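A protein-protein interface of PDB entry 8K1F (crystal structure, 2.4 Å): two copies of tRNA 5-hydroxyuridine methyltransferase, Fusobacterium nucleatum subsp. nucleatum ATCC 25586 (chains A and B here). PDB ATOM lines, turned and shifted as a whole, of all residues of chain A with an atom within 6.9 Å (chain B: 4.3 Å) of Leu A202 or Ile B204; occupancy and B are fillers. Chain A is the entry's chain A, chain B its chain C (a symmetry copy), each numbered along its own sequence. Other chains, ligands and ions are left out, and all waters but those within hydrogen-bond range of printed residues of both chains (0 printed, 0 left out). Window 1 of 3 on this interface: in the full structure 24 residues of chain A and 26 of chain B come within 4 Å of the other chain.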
ATOM      1  N   ILE A  12     -33.634 -21.388   2.171  1.00  0.00           N
ATOM      2  CA  ILE A  12     -32.374 -20.859   1.662  1.00  0.00           C
ATOM      3  C   ILE A  12     -31.791 -21.771   0.583  1.00  0.00           C
ATOM      4  O   ILE A  12     -31.331 -21.305  -0.468  1.00  0.00           O
ATOM      5  CB  ILE A  12     -31.393 -20.652   2.823  1.00  0.00           C
ATOM      6  CG1 ILE A  12     -32.056 -19.787   3.904  1.00  0.00           C
ATOM      7  CG2 ILE A  12     -30.111 -20.034   2.307  1.00  0.00           C
ATOM      8  CD1 ILE A  12     -31.240 -19.673   5.194  1.00  0.00           C
ATOM      9  N   TYR A  49     -21.592 -19.366   1.808  1.00  0.00           N
ATOM     10  CA  TYR A  49     -21.057 -18.388   2.751  1.00  0.00           C
ATOM     11  C   TYR A  49     -19.539 -18.342   2.665  1.00  0.00           C
ATOM     12  O   TYR A  49     -18.933 -17.260   2.694  1.00  0.00           O
ATOM     13  CB  TYR A  49     -21.523 -18.758   4.157  1.00  0.00           C
ATOM     14  CG  TYR A  49     -21.175 -17.792   5.249  1.00  0.00           C
ATOM     15  CD1 TYR A  49     -21.312 -16.417   5.076  1.00  0.00           C
ATOM     16  CD2 TYR A  49     -20.732 -18.257   6.470  1.00  0.00           C
ATOM     17  CE1 TYR A  49     -20.993 -15.528   6.106  1.00  0.00           C
ATOM     18  CE2 TYR A  49     -20.423 -17.389   7.501  1.00  0.00           C
ATOM     19  CZ  TYR A  49     -20.556 -16.031   7.316  1.00  0.00           C
ATOM     20  OH  TYR A  49     -20.243 -15.199   8.358  1.00  0.00           O
ATOM     21  N   ILE A  53     -17.419 -14.981   1.928  1.00  0.00           N
ATOM     22  CA  ILE A  53     -16.377 -14.429   2.792  1.00  0.00           C
ATOM     23  C   ILE A  53     -15.111 -14.188   1.996  1.00  0.00           C
ATOM     24  O   ILE A  53     -14.431 -13.164   2.174  1.00  0.00           O
ATOM     25  CB  ILE A  53     -16.110 -15.365   3.984  1.00  0.00           C
ATOM     26  CG1 ILE A  53     -17.297 -15.340   4.951  1.00  0.00           C
ATOM     27  CG2 ILE A  53     -14.833 -14.947   4.681  1.00  0.00           C
ATOM     28  CD1 ILE A  53     -17.282 -16.448   5.955  1.00  0.00           C
ATOM     29  N   ILE A 165     -19.188 -27.058  14.062  1.00  0.00           N
ATOM     30  CA  ILE A 165     -18.648 -26.786  15.390  1.00  0.00           C
ATOM     31  C   ILE A 165     -19.651 -27.071  16.500  1.00  0.00           C
ATOM     32  O   ILE A 165     -19.246 -27.234  17.653  1.00  0.00           O
ATOM     33  CB  ILE A 165     -18.150 -25.334  15.476  1.00  0.00           C
ATOM     34  CG1 ILE A 165     -17.081 -25.205  16.566  1.00  0.00           C
ATOM     35  CG2 ILE A 165     -19.315 -24.391  15.691  1.00  0.00           C
ATOM     36  CD1 ILE A 165     -16.296 -23.959  16.471  1.00  0.00           C
ATOM     37  N   LEU A 166     -20.940 -27.142  16.184  1.00  0.00           N
ATOM     38  CA  LEU A 166     -21.986 -27.379  17.167  1.00  0.00           C
ATOM     39  C   LEU A 166     -22.293 -28.864  17.274  1.00  0.00           C
ATOM     40  O   LEU A 166     -23.070 -29.400  16.479  1.00  0.00           O
ATOM     41  CB  LEU A 166     -23.256 -26.619  16.787  1.00  0.00           C
ATOM     42  CG  LEU A 166     -23.222 -25.088  16.788  1.00  0.00           C
ATOM     43  CD1 LEU A 166     -24.538 -24.522  16.243  1.00  0.00           C
ATOM     44  CD2 LEU A 166     -22.939 -24.554  18.189  1.00  0.00           C
ATOM     45  N   TYR A 194     -14.040 -18.789  22.983  1.00  0.00           N
ATOM     46  CA  TYR A 194     -14.698 -17.607  23.537  1.00  0.00           C
ATOM     47  C   TYR A 194     -13.842 -16.928  24.602  1.00  0.00           C
ATOM     48  O   TYR A 194     -13.842 -15.699  24.698  1.00  0.00           O
ATOM     49  CB  TYR A 194     -16.063 -17.988  24.114  1.00  0.00           C
ATOM     50  CG  TYR A 194     -17.269 -17.797  23.187  1.00  0.00           C
ATOM     51  CD1 TYR A 194     -17.646 -16.532  22.734  1.00  0.00           C
ATOM     52  CD2 TYR A 194     -18.061 -18.886  22.806  1.00  0.00           C
ATOM     53  CE1 TYR A 194     -18.759 -16.356  21.895  1.00  0.00           C
ATOM     54  CE2 TYR A 194     -19.191 -18.718  21.967  1.00  0.00           C
ATOM     55  CZ  TYR A 194     -19.530 -17.454  21.517  1.00  0.00           C
ATOM     56  OH  TYR A 194     -20.629 -17.296  20.697  1.00  0.00           O
ATOM     57  N   PHE A 199     -14.277 -14.220  18.411  1.00  0.00           N
ATOM     58  CA  PHE A 199     -14.965 -15.434  17.986  1.00  0.00           C
ATOM     59  C   PHE A 199     -16.467 -15.161  17.953  1.00  0.00           C
ATOM     60  O   PHE A 199     -16.989 -14.491  18.851  1.00  0.00           O
ATOM     61  CB  PHE A 199     -14.601 -16.575  18.952  1.00  0.00           C
ATOM     62  CG  PHE A 199     -15.293 -17.875  18.670  1.00  0.00           C
ATOM     63  CD1 PHE A 199     -15.123 -18.526  17.457  1.00  0.00           C
ATOM     64  CD2 PHE A 199     -16.094 -18.470  19.640  1.00  0.00           C
ATOM     65  CE1 PHE A 199     -15.772 -19.746  17.206  1.00  0.00           C
ATOM     66  CE2 PHE A 199     -16.731 -19.667  19.396  1.00  0.00           C
ATOM     67  CZ  PHE A 199     -16.578 -20.302  18.174  1.00  0.00           C
ATOM     68  N   VAL A 200     -17.139 -15.593  16.877  1.00  0.00           N
ATOM     69  CA  VAL A 200     -18.599 -15.671  16.803  1.00  0.00           C
ATOM     70  C   VAL A 200     -18.987 -17.118  16.580  1.00  0.00           C
ATOM     71  O   VAL A 200     -18.296 -17.866  15.885  1.00  0.00           O
ATOM     72  CB  VAL A 200     -19.264 -14.823  15.685  1.00  0.00           C
ATOM     73  CG1 VAL A 200     -19.442 -13.396  16.102  1.00  0.00           C
ATOM     74  CG2 VAL A 200     -18.500 -14.941  14.362  1.00  0.00           C
ATOM     75  N   LEU A 201     -20.145 -17.457  17.101  1.00  0.00           N
ATOM     76  CA  LEU A 201     -20.773 -18.762  16.857  1.00  0.00           C
ATOM     77  C   LEU A 201     -21.959 -18.482  15.937  1.00  0.00           C
ATOM     78  O   LEU A 201     -22.709 -17.608  16.219  1.00  0.00           O
ATOM     79  CB  LEU A 201     -21.182 -19.401  18.181  1.00  0.00           C
ATOM     80  CG  LEU A 201     -21.082 -20.918  18.234  1.00  0.00           C
ATOM     81  CD1 LEU A 201     -19.854 -21.418  17.515  1.00  0.00           C
ATOM     82  CD2 LEU A 201     -21.100 -21.418  19.656  1.00  0.00           C
ATOM     83  N   LEU A 202     -22.053 -19.189  14.836  1.00  0.00           N
ATOM     84  CA  LEU A 202     -23.161 -18.974  13.885  1.00  0.00           C
ATOM     85  C   LEU A 202     -23.967 -20.253  13.721  1.00  0.00           C
ATOM     86  O   LEU A 202     -23.404 -21.266  13.450  1.00  0.00           O
ATOM     87  CB  LEU A 202     -22.601 -18.499  12.542  1.00  0.00           C
ATOM     88  CG  LEU A 202     -22.074 -17.071  12.537  1.00  0.00           C
ATOM     89  CD1 LEU A 202     -21.519 -16.663  11.194  1.00  0.00           C
ATOM     90  CD2 LEU A 202     -23.147 -16.116  12.987  1.00  0.00           C
ATOM     91  N   PRO A 203     -25.301 -20.225  13.783  1.00  0.00           N
ATOM     92  CA  PRO A 203     -26.084 -21.416  13.544  1.00  0.00           C
ATOM     93  C   PRO A 203     -26.336 -21.758  12.064  1.00  0.00           C
ATOM     94  O   PRO A 203     -27.419 -22.043  11.736  1.00  0.00           O
ATOM     95  CB  PRO A 203     -27.374 -21.072  14.260  1.00  0.00           C
ATOM     96  CG  PRO A 203     -27.509 -19.628  14.007  1.00  0.00           C
ATOM     97  CD  PRO A 203     -26.111 -19.088  14.127  1.00  0.00           C
ATOM     98  N   ILE A 204     -25.288 -21.711  11.263  1.00  0.00           N
ATOM     99  CA  ILE A 204     -25.393 -22.091   9.837  1.00  0.00           C
ATOM    100  C   ILE A 204     -25.157 -23.589   9.755  1.00  0.00           C
ATOM    101  O   ILE A 204     -24.207 -24.038  10.336  1.00  0.00           O
ATOM    102  CB  ILE A 204     -24.394 -21.331   8.967  1.00  0.00           C
ATOM    103  CG1 ILE A 204     -24.652 -19.835   9.017  1.00  0.00           C
ATOM    104  CG2 ILE A 204     -24.457 -21.871   7.557  1.00  0.00           C
ATOM    105  CD1 ILE A 204     -23.604 -19.040   8.367  1.00  0.00           C
ATOM    106  N   SER A 205     -26.024 -24.289   9.057  1.00  0.00           N
ATOM    107  CA  SER A 205     -25.915 -25.752   8.902  1.00  0.00           C
ATOM    108  C   SER A 205     -25.696 -26.431  10.254  1.00  0.00           C
ATOM    109  O   SER A 205     -26.579 -26.419  11.059  1.00  0.00           O
ATOM    110  CB  SER A 205     -24.834 -26.102   7.952  1.00  0.00           C
ATOM    111  OG  SER A 205     -25.291 -26.086   6.635  1.00  0.00           O
ATOM    112  N   ASP A 206     -24.496 -26.948  10.462  1.00  0.00           N
ATOM    113  CA  ASP A 206     -24.169 -27.698  11.690  1.00  0.00           C
ATOM    114  C   ASP A 206     -23.233 -26.905  12.590  1.00  0.00           C
ATOM    115  O   ASP A 206     -22.537 -27.511  13.339  1.00  0.00           O
ATOM    116  CB  ASP A 206     -23.560 -29.046  11.349  1.00  0.00           C
ATOM    117  CG  ASP A 206     -24.555 -30.179  11.344  1.00  0.00           C
ATOM    118  OD1 ASP A 206     -25.722 -29.936  11.475  1.00  0.00           O
ATOM    119  OD2 ASP A 206     -24.115 -31.295  11.200  1.00  0.00           O
ATOM    120  N   GLY A 207     -23.266 -25.590  12.498  1.00  0.00           N
ATOM    121  CA  GLY A 207     -22.404 -24.749  13.326  1.00  0.00           C
ATOM    122  C   GLY A 207     -21.234 -24.161  12.577  1.00  0.00           C
ATOM    123  O   GLY A 207     -20.548 -24.864  11.924  1.00  0.00           O
ATOM    124  N   VAL A 208     -21.068 -22.863  12.669  1.00  0.00           N
ATOM    125  CA  VAL A 208     -19.865 -22.257  12.068  1.00  0.00           C
ATOM    126  C   VAL A 208     -19.178 -21.393  13.110  1.00  0.00           C
ATOM    127  O   VAL A 208     -19.789 -20.566  13.688  1.00  0.00           O
ATOM    128  CB  VAL A 208     -20.120 -21.507  10.760  1.00  0.00           C
ATOM    129  CG1 VAL A 208     -18.885 -20.755  10.337  1.00  0.00           C
ATOM    130  CG2 VAL A 208     -20.504 -22.479   9.690  1.00  0.00           C
ATOM    131  N   GLY A 209     -17.926 -21.660  13.335  1.00  0.00           N
ATOM    132  CA  GLY A 209     -17.152 -20.823  14.273  1.00  0.00           C
ATOM    133  C   GLY A 209     -16.129 -19.972  13.540  1.00  0.00           C
ATOM    134  O   GLY A 209     -15.212 -20.552  12.925  1.00  0.00           O
ATOM    135  N   ILE A 210     -16.281 -18.645  13.603  1.00  0.00           N
ATOM    136  CA  ILE A 210     -15.364 -17.733  12.928  1.00  0.00           C
ATOM    137  C   ILE A 210     -14.448 -17.104  13.971  1.00  0.00           C
ATOM    138  O   ILE A 210     -14.923 -16.462  14.916  1.00  0.00           O
ATOM    139  CB  ILE A 210     -16.103 -16.640  12.145  1.00  0.00           C
ATOM    140  CG1 ILE A 210     -17.144 -17.227  11.211  1.00  0.00           C
ATOM    141  CG2 ILE A 210     -15.099 -15.834  11.320  1.00  0.00           C
ATOM    142  CD1 ILE A 210     -16.523 -17.843  10.006  1.00  0.00           C
ATOM    143  N   ILE B  12     -25.969 -21.198  21.748  1.00  0.00           N
ATOM    144  CA  ILE B  12     -25.223 -19.988  21.407  1.00  0.00           C
ATOM    145  C   ILE B  12     -25.574 -18.865  22.378  1.00  0.00           C
ATOM    146  O   ILE B  12     -24.693 -18.270  23.010  1.00  0.00           O
ATOM    147  CB  ILE B  12     -25.491 -19.578  19.948  1.00  0.00           C
ATOM    148  CG1 ILE B  12     -24.939 -20.627  18.980  1.00  0.00           C
ATOM    149  CG2 ILE B  12     -24.852 -18.243  19.663  1.00  0.00           C
ATOM    150  CD1 ILE B  12     -25.471 -20.494  17.563  1.00  0.00           C
ATOM    151  N   GLU B  45     -27.952 -12.987  19.513  1.00  0.00           N
ATOM    152  CA  GLU B  45     -27.182 -13.534  18.401  1.00  0.00           C
ATOM    153  C   GLU B  45     -26.909 -12.459  17.357  1.00  0.00           C
ATOM    154  O   GLU B  45     -25.808 -12.392  16.794  1.00  0.00           O
ATOM    155  CB  GLU B  45     -27.941 -14.696  17.760  1.00  0.00           C
ATOM    156  CG  GLU B  45     -27.691 -16.073  18.323  1.00  0.00           C
ATOM    157  CD  GLU B  45     -28.137 -17.156  17.336  1.00  0.00           C
ATOM    158  OE1 GLU B  45     -29.275 -17.072  16.796  1.00  0.00           O
ATOM    159  OE2 GLU B  45     -27.339 -18.084  17.079  1.00  0.00           O
ATOM    160  N   TYR B  49     -23.143 -10.655  16.297  1.00  0.00           N
ATOM    161  CA  TYR B  49     -22.715 -10.774  14.909  1.00  0.00           C
ATOM    162  C   TYR B  49     -22.448  -9.397  14.318  1.00  0.00           C
ATOM    163  O   TYR B  49     -21.351  -9.117  13.821  1.00  0.00           O
ATOM    164  CB  TYR B  49     -23.780 -11.528  14.114  1.00  0.00           C
ATOM    165  CG  TYR B  49     -23.404 -11.848  12.683  1.00  0.00           C
ATOM    166  CD1 TYR B  49     -22.218 -12.514  12.378  1.00  0.00           C
ATOM    167  CD2 TYR B  49     -24.246 -11.496  11.632  1.00  0.00           C
ATOM    168  CE1 TYR B  49     -21.880 -12.811  11.058  1.00  0.00           C
ATOM    169  CE2 TYR B  49     -23.921 -11.800  10.310  1.00  0.00           C
ATOM    170  CZ  TYR B  49     -22.740 -12.454  10.033  1.00  0.00           C
ATOM    171  OH  TYR B  49     -22.416 -12.739   8.721  1.00  0.00           O
ATOM    172  N   LEU B 202     -28.516 -15.833   5.480  1.00  0.00           N
ATOM    173  CA  LEU B 202     -28.033 -16.549   6.658  1.00  0.00           C
ATOM    174  C   LEU B 202     -29.172 -16.814   7.638  1.00  0.00           C
ATOM    175  O   LEU B 202     -29.900 -15.877   8.022  1.00  0.00           O
ATOM    176  CB  LEU B 202     -26.923 -15.766   7.343  1.00  0.00           C
ATOM    177  CG  LEU B 202     -25.689 -15.602   6.465  1.00  0.00           C
ATOM    178  CD1 LEU B 202     -24.593 -14.859   7.230  1.00  0.00           C
ATOM    179  CD2 LEU B 202     -25.218 -16.975   5.962  1.00  0.00           C
ATOM    180  N   PRO B 203     -29.351 -18.063   8.070  1.00  0.00           N
ATOM    181  CA  PRO B 203     -30.405 -18.396   9.043  1.00  0.00           C
ATOM    182  C   PRO B 203     -29.988 -18.083  10.476  1.00  0.00           C
ATOM    183  O   PRO B 203     -29.987 -18.951  11.353  1.00  0.00           O
ATOM    184  CB  PRO B 203     -30.595 -19.898   8.810  1.00  0.00           C
ATOM    185  CG  PRO B 203     -29.207 -20.373   8.456  1.00  0.00           C
ATOM    186  CD  PRO B 203     -28.497 -19.227   7.765  1.00  0.00           C
ATOM    187  N   ILE B 204     -29.602 -16.831  10.721  1.00  0.00           N
ATOM    188  CA  ILE B 204     -29.356 -16.354  12.077  1.00  0.00           C
ATOM    189  C   ILE B 204     -30.622 -15.687  12.583  1.00  0.00           C
ATOM    190  O   ILE B 204     -31.200 -14.845  11.884  1.00  0.00           O
ATOM    191  CB  ILE B 204     -28.180 -15.371  12.117  1.00  0.00           C
ATOM    192  CG1 ILE B 204     -26.885 -16.067  11.680  1.00  0.00           C
ATOM    193  CG2 ILE B 204     -28.067 -14.756  13.513  1.00  0.00           C
ATOM    194  CD1 ILE B 204     -25.947 -15.195  10.833  1.00  0.00           C
ATOM    195  N   SER B 205     -31.044 -16.040  13.798  1.00  0.00           N
ATOM    196  CA  SER B 205     -32.234 -15.444  14.410  1.00  0.00           C
ATOM    197  C   SER B 205     -33.405 -15.440  13.422  1.00  0.00           C
ATOM    198  O   SER B 205     -33.820 -16.503  12.959  1.00  0.00           O
ATOM    199  CB  SER B 205     -31.905 -14.037  14.918  1.00  0.00           C
ATOM    200  OG  SER B 205     -32.977 -13.510  15.679  1.00  0.00           O
ATOM    201  N   ASP B 206     -33.919 -14.272  13.043  1.00  0.00           N
ATOM    202  CA  ASP B 206     -35.069 -14.197  12.148  1.00  0.00           C
ATOM    203  C   ASP B 206     -34.679 -13.968  10.691  1.00  0.00           C
ATOM    204  O   ASP B 206     -35.544 -13.622   9.867  1.00  0.00           O
ATOM    205  CB  ASP B 206     -36.022 -13.090  12.597  1.00  0.00           C
ATOM    206  CG  ASP B 206     -37.090 -13.582  13.548  1.00  0.00           C
ATOM    207  OD1 ASP B 206     -37.725 -14.609  13.239  1.00  0.00           O
ATOM    208  OD2 ASP B 206     -37.305 -12.929  14.594  1.00  0.00           O
ATOM    209  N   GLY B 207     -33.407 -14.137  10.355  1.00  0.00           N
ATOM    210  CA  GLY B 207     -32.996 -14.022   8.971  1.00  0.00           C
ATOM    211  C   GLY B 207     -32.141 -12.805   8.720  1.00  0.00           C
ATOM    212  O   GLY B 207     -32.488 -11.691   9.133  1.00  0.00           O
ATOM    213  N   VAL B 208     -31.012 -12.997   8.047  1.00  0.00           N
ATOM    214  CA  VAL B 208     -30.051 -11.925   7.834  1.00  0.00           C
ATOM    215  C   VAL B 208     -29.633 -11.916   6.365  1.00  0.00           C
ATOM    216  O   VAL B 208     -29.204 -12.946   5.830  1.00  0.00           O
ATOM    217  CB  VAL B 208     -28.834 -12.075   8.756  1.00  0.00           C
ATOM    218  CG1 VAL B 208     -27.791 -11.033   8.426  1.00  0.00           C
ATOM    219  CG2 VAL B 208     -29.258 -11.964  10.215  1.00  0.00           C
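The side-chain hydroxyl of Tyr A49 is in hydrogen-bond range of the side-chain hydroxyl of Tyr B49.
Of the 18 printed residues of chain A, 6 touch a printed residue of chain B. Among the printed residues, 11 pairs touch across the chains. Among the printed residues, no Asp or Glu carboxylate lies within 4 Å of a Lys or Arg side-chain nitrogen of the other chain.
Leu A202 touches just these residues of chain B: Tyr B49 (3.8 Å) and Ile B204 (3.7 Å). Ile B204 touches two residues of chain A. Printed residues of chain A within 4 Å of Ile B12: Leu A201 and Pro A203. Printed residues of chain A within 4 Å of Pro B203: Ile A12 (3.7 Å) and Pro A203 (3.7 Å). Of the printed residues of chain B, Ile A204 touches Leu B202. Printed residues of chain B within 4 Å of Tyr A49: Tyr B49 (3.3 Å) and Leu B202 (3.8 Å). Printed residues of chain B within 4 Å of Leu A201: Ile B12.
Ile A12 touches Pro B203, and with the chains exchanged Pro A203 touches Ile B12. Tyr A49 touches Leu B202, and with the chains exchanged Leu A202 touches Tyr B49. Leu A202 touches Ile B204, and with the chains exchanged Ile A204 touches Leu B202. Pro A203 touches Ile B204, but with the chains exchanged Ile A204 does not touch Pro B203 (4.1 Å). 9 positions are printed for both chains.
Among the printed residues, merely in contact across the chains: Pro A203 with Glu B45, Ile A204 with Leu B202, Leu A202 with Ile B204, Ile A12 with Pro B203, Pro A203 with Pro B203, Pro A203 with Ile B12, Leu A202 with Tyr B49, Tyr A49 with Leu B202, Leu A201 with Ile B12 and Pro A203 with Ile B204.
N of Leu B202 lies within hydrogen-bond range of O of Val B208, 3.0 Å away. The backbone NH of Leu A202 lies within hydrogen-bond range of the backbone carbonyl oxygen of Val A208 (2.9 Å).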
